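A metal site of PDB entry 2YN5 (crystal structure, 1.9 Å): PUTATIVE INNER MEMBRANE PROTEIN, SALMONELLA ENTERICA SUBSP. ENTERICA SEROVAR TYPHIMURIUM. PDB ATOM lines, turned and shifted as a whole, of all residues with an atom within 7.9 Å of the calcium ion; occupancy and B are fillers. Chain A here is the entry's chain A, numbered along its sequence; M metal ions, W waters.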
ATOM      1  N   ILE A 103      34.573 -19.940   1.126  1.00  0.00           N
ATOM      2  CA  ILE A 103      33.716 -19.831   2.297  1.00  0.00           C
ATOM      3  C   ILE A 103      33.840 -21.189   3.000  1.00  0.00           C
ATOM      4  O   ILE A 103      33.730 -22.223   2.356  1.00  0.00           O
ATOM      5  CB  ILE A 103      32.247 -19.564   1.884  1.00  0.00           C
ATOM      6  CG1 ILE A 103      32.124 -18.205   1.181  1.00  0.00           C
ATOM      7  CG2 ILE A 103      31.319 -19.570   3.103  1.00  0.00           C
ATOM      8  CD1 ILE A 103      30.810 -18.052   0.424  1.00  0.00           C
ATOM      9  N   ASP A 152      33.776 -16.030  13.183  1.00  0.00           N
ATOM     10  CA  ASP A 152      33.011 -15.889  11.940  1.00  0.00           C
ATOM     11  C   ASP A 152      33.207 -14.507  11.333  1.00  0.00           C
ATOM     12  O   ASP A 152      33.229 -13.534  12.073  1.00  0.00           O
ATOM     13  CB  ASP A 152      31.503 -16.134  12.189  1.00  0.00           C
ATOM     14  CG  ASP A 152      31.128 -17.605  12.109  1.00  0.00           C
ATOM     15  OD1 ASP A 152      31.953 -18.451  12.489  1.00  0.00           O
ATOM     16  OD2 ASP A 152      29.986 -17.905  11.680  1.00  0.00           O
ATOM     17  N   ILE A 178      34.655 -17.124   7.037  1.00  0.00           N
ATOM     18  CA  ILE A 178      34.441 -18.166   8.033  1.00  0.00           C
ATOM     19  C   ILE A 178      32.960 -18.087   8.464  1.00  0.00           C
ATOM     20  O   ILE A 178      32.473 -17.066   8.903  1.00  0.00           O
ATOM     21  CB  ILE A 178      35.405 -18.012   9.242  1.00  0.00           C
ATOM     22  CG1 ILE A 178      36.883 -18.032   8.798  1.00  0.00           C
ATOM     23  CG2 ILE A 178      35.136 -19.069  10.298  1.00  0.00           C
ATOM     24  CD1 ILE A 178      37.378 -19.296   8.117  1.00  0.00           C
ATOM     25  N   ASP A 179      32.252 -19.193   8.328  1.00  0.00           N
ATOM     26  CA  ASP A 179      30.829 -19.222   8.617  1.00  0.00           C
ATOM     27  C   ASP A 179      30.594 -20.566   9.281  1.00  0.00           C
ATOM     28  O   ASP A 179      30.572 -21.598   8.609  1.00  0.00           O
ATOM     29  CB  ASP A 179      30.007 -19.093   7.334  1.00  0.00           C
ATOM     30  CG  ASP A 179      28.490 -19.245   7.570  1.00  0.00           C
ATOM     31  OD1 ASP A 179      28.038 -19.608   8.684  1.00  0.00           O
ATOM     32  OD2 ASP A 179      27.729 -19.037   6.616  1.00  0.00           O
ATOM     33  N   SER A 180      30.461 -20.509  10.605  1.00  0.00           N
ATOM     34  CA  SER A 180      30.142 -21.686  11.391  1.00  0.00           C
ATOM     35  C   SER A 180      28.754 -21.513  12.062  1.00  0.00           C
ATOM     36  O   SER A 180      28.353 -22.321  12.932  1.00  0.00           O
ATOM     37  CB  SER A 180      31.230 -21.899  12.452  1.00  0.00           C
ATOM     38  OG  SER A 180      31.289 -20.762  13.304  1.00  0.00           O
ATOM     39  N   THR A 181      28.011 -20.473  11.642  1.00  0.00           N
ATOM     40  CA  THR A 181      26.742 -20.095  12.308  1.00  0.00           C
ATOM     41  C   THR A 181      25.527 -20.485  11.470  1.00  0.00           C
ATOM     42  O   THR A 181      25.522 -20.311  10.252  1.00  0.00           O
ATOM     43  CB  THR A 181      26.714 -18.580  12.618  1.00  0.00           C
ATOM     44  OG1 THR A 181      27.949 -18.210  13.231  1.00  0.00           O
ATOM     45  CG2 THR A 181      25.581 -18.219  13.583  1.00  0.00           C
ATOM     46  N   LEU A 182      24.510 -21.062  12.116  1.00  0.00           N
ATOM     47  CA  LEU A 182      23.257 -21.343  11.426  1.00  0.00           C
ATOM     48  C   LEU A 182      22.134 -21.413  12.455  1.00  0.00           C
ATOM     49  O   LEU A 182      22.194 -22.197  13.396  1.00  0.00           O
ATOM     50  CB  LEU A 182      23.345 -22.645  10.625  1.00  0.00           C
ATOM     51  CG  LEU A 182      22.153 -23.174   9.796  1.00  0.00           C
ATOM     52  CD1 LEU A 182      21.633 -22.181   8.765  1.00  0.00           C
ATOM     53  CD2 LEU A 182      22.551 -24.460   9.097  1.00  0.00           C
ATOM     54  N   THR A 183      21.116 -20.582  12.257  1.00  0.00           N
ATOM     55  CA  THR A 183      19.962 -20.525  13.141  1.00  0.00           C
ATOM     56  C   THR A 183      19.230 -21.863  13.071  1.00  0.00           C
ATOM     57  O   THR A 183      19.019 -22.419  11.989  1.00  0.00           O
ATOM     58  CB  THR A 183      18.985 -19.418  12.726  1.00  0.00           C
ATOM     59  OG1 THR A 183      19.687 -18.171  12.576  1.00  0.00           O
ATOM     60  CG2 THR A 183      17.853 -19.266  13.764  1.00  0.00           C
ATOM     61  N   ASP A 217      17.801 -19.146   7.621  1.00  0.00           N
ATOM     62  CA  ASP A 217      18.805 -18.115   7.275  1.00  0.00           C
ATOM     63  C   ASP A 217      18.891 -17.900   5.761  1.00  0.00           C
ATOM     64  O   ASP A 217      18.676 -18.818   4.958  1.00  0.00           O
ATOM     65  CB  ASP A 217      20.189 -18.442   7.892  1.00  0.00           C
ATOM     66  CG  ASP A 217      20.234 -18.229   9.417  1.00  0.00           C
ATOM     67  OD1 ASP A 217      19.287 -17.638   9.982  1.00  0.00           O
ATOM     68  OD2 ASP A 217      21.224 -18.646  10.075  1.00  0.00           O
ATOM     69  N   ALA A 218      19.203 -16.664   5.347  1.00  0.00           N
ATOM     70  CA  ALA A 218      19.256 -16.332   3.923  1.00  0.00           C
ATOM     71  C   ALA A 218      20.285 -17.135   3.101  1.00  0.00           C
ATOM     72  O   ALA A 218      20.141 -17.231   1.886  1.00  0.00           O
ATOM     73  CB  ALA A 218      19.478 -14.834   3.725  1.00  0.00           C
ATOM     74  N   ASP A 219      21.303 -17.710   3.753  1.00  0.00           N
ATOM     75  CA  ASP A 219      22.353 -18.495   3.084  1.00  0.00           C
ATOM     76  C   ASP A 219      22.095 -20.026   3.117  1.00  0.00           C
ATOM     77  O   ASP A 219      23.020 -20.818   2.922  1.00  0.00           O
ATOM     78  CB  ASP A 219      23.747 -18.211   3.681  1.00  0.00           C
ATOM     79  CG  ASP A 219      23.810 -18.578   5.175  1.00  0.00           C
ATOM     80  OD1 ASP A 219      22.755 -18.576   5.845  1.00  0.00           O
ATOM     81  OD2 ASP A 219      24.906 -18.906   5.680  1.00  0.00           O
ATOM     82  N   VAL A 220      20.856 -20.406   3.384  1.00  0.00           N
ATOM     83  CA  VAL A 220      20.461 -21.807   3.311  1.00  0.00           C
ATOM     84  C   VAL A 220      20.378 -22.281   1.856  1.00  0.00           C
ATOM     85  O   VAL A 220      19.806 -21.604   0.995  1.00  0.00           O
ATOM     86  CB  VAL A 220      19.155 -22.034   4.108  1.00  0.00           C
ATOM     87  CG1 VAL A 220      18.543 -23.382   3.780  1.00  0.00           C
ATOM     88  CG2 VAL A 220      19.454 -21.943   5.603  1.00  0.00           C
ATOM     89  N   VAL A 265      20.632 -26.765   5.607  1.00  0.00           N
ATOM     90  CA  VAL A 265      22.074 -26.730   5.388  1.00  0.00           C
ATOM     91  C   VAL A 265      22.399 -25.427   4.671  1.00  0.00           C
ATOM     92  O   VAL A 265      21.674 -25.005   3.766  1.00  0.00           O
ATOM     93  CB  VAL A 265      22.584 -27.970   4.640  1.00  0.00           C
ATOM     94  CG1 VAL A 265      24.062 -27.830   4.263  1.00  0.00           C
ATOM     95  CG2 VAL A 265      22.421 -29.207   5.520  1.00  0.00           C
ATOM     96  N   ASP A 266      23.435 -24.743   5.137  1.00  0.00           N
ATOM     97  CA  ASP A 266      23.840 -23.468   4.526  1.00  0.00           C
ATOM     98  C   ASP A 266      24.953 -23.714   3.518  1.00  0.00           C
ATOM     99  O   ASP A 266      25.397 -24.861   3.367  1.00  0.00           O
ATOM    100  CB  ASP A 266      24.123 -22.363   5.581  1.00  0.00           C
ATOM    101  CG  ASP A 266      25.454 -22.522   6.325  1.00  0.00           C
ATOM    102  OD1 ASP A 266      26.275 -23.383   5.947  1.00  0.00           O
ATOM    103  OD2 ASP A 266      25.660 -21.774   7.320  1.00  0.00           O
ATOM    104  N   ARG A 267      25.373 -22.679   2.805  1.00  0.00           N
ATOM    105  CA  ARG A 267      26.402 -22.830   1.751  1.00  0.00           C
ATOM    106  C   ARG A 267      27.760 -23.289   2.306  1.00  0.00           C
ATOM    107  O   ARG A 267      28.544 -23.882   1.575  1.00  0.00           O
ATOM    108  CB  ARG A 267      26.575 -21.508   1.021  1.00  0.00           C
ATOM    109  CG  ARG A 267      26.898 -20.399   1.990  1.00  0.00           C
ATOM    110  CD  ARG A 267      27.068 -19.062   1.298  1.00  0.00           C
ATOM    111  NE  ARG A 267      27.488 -18.097   2.307  1.00  0.00           N
ATOM    112  CZ  ARG A 267      27.717 -16.805   2.060  1.00  0.00           C
ATOM    113  NH1 ARG A 267      27.574 -16.304   0.844  1.00  0.00           N
ATOM    114  NH2 ARG A 267      28.111 -16.026   3.063  1.00  0.00           N
ATOM    115  N   ALA A 268      28.027 -23.006   3.577  1.00  0.00           N
ATOM    116  CA  ALA A 268      29.260 -23.441   4.243  1.00  0.00           C
ATOM    117  C   ALA A 268      29.206 -24.917   4.708  1.00  0.00           C
ATOM    118  O   ALA A 268      30.205 -25.483   5.195  1.00  0.00           O
ATOM    119  CB  ALA A 268      29.573 -22.525   5.423  1.00  0.00           C
ATOM    120  N   GLY A 269      28.052 -25.549   4.548  1.00  0.00           N
ATOM    121  CA  GLY A 269      27.902 -26.945   4.976  1.00  0.00           C
ATOM    122  C   GLY A 269      27.508 -27.135   6.437  1.00  0.00           C
ATOM    123  O   GLY A 269      27.463 -28.274   6.928  1.00  0.00           O
ATOM    124  N   ASN A 270      27.216 -26.042   7.140  1.00  0.00           N
ATOM    125  CA  ASN A 270      26.616 -26.144   8.481  1.00  0.00           C
ATOM    126  C   ASN A 270      25.239 -26.796   8.358  1.00  0.00           C
ATOM    127  O   ASN A 270      24.534 -26.598   7.366  1.00  0.00           O
ATOM    128  CB  ASN A 270      26.490 -24.783   9.156  1.00  0.00           C
ATOM    129  CG  ASN A 270      27.851 -24.108   9.382  1.00  0.00           C
ATOM    130  OD1 ASN A 270      28.748 -24.645  10.073  1.00  0.00           O
ATOM    131  ND2 ASN A 270      28.037 -22.946   8.768  1.00  0.00           N
HETATM  132 CA    CA M   1      25.718 -19.554   7.952  1.00  0.00          CA
HETATM  133  O   HOH W   1      26.063 -17.396   8.755  1.00  0.00           O
HETATM  134  O   HOH W   2      23.381 -19.195   8.226  1.00  0.00           O
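The calcium ion is bound by the side-chain carboxylate (OD2) of Asp 266 (2.3 Å), water W1 (2.3 Å), water W2 (2.4 Å), the backbone carbonyl oxygen (O) of Thr 181 (2.4 Å), the side-chain carboxylate (OD1) of Asp 179 (2.4 Å), the side-chain carboxylate (OD2) of Asp 179 (2.5 Å) and the side-chain carboxylate (OD2) of Asp 219 (2.5 Å).
The side-chain carboxylate (OD1) of Asp 266 sits at hydrogen-bond distance from the backbone NH (N) of Ala 268 (3.0 Å). The backbone carbonyl oxygen (O) of Asp 219 is in hydrogen-bond range of the backbone NH (N) of Arg 267 (3.0 Å). O of Asp 179 lies within hydrogen-bond range of ND2 of Asn 270 (2.9 Å). OD1 of Asp 266 is in hydrogen-bond range of N of Asn 270 (3.1 Å). The side-chain carboxylate (OD2) of Asp 152 lies within hydrogen-bond range of the side-chain hydroxyl (OG1) of Thr 181 (2.6 Å). N of Gly 269 sits at hydrogen-bond distance from OD1 of Asp 266.
Water W2 bridges OD1 of Asp 219 (2.5 Å) and OD2 of Asp 217 (2.9 Å).
Within 4 Å of the calcium ion: Asp 179, Thr 181, Asp 219 and Asp 266. The nearest printed residue that does not touch the calcium ion is Asn 270 (4.2 Å).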
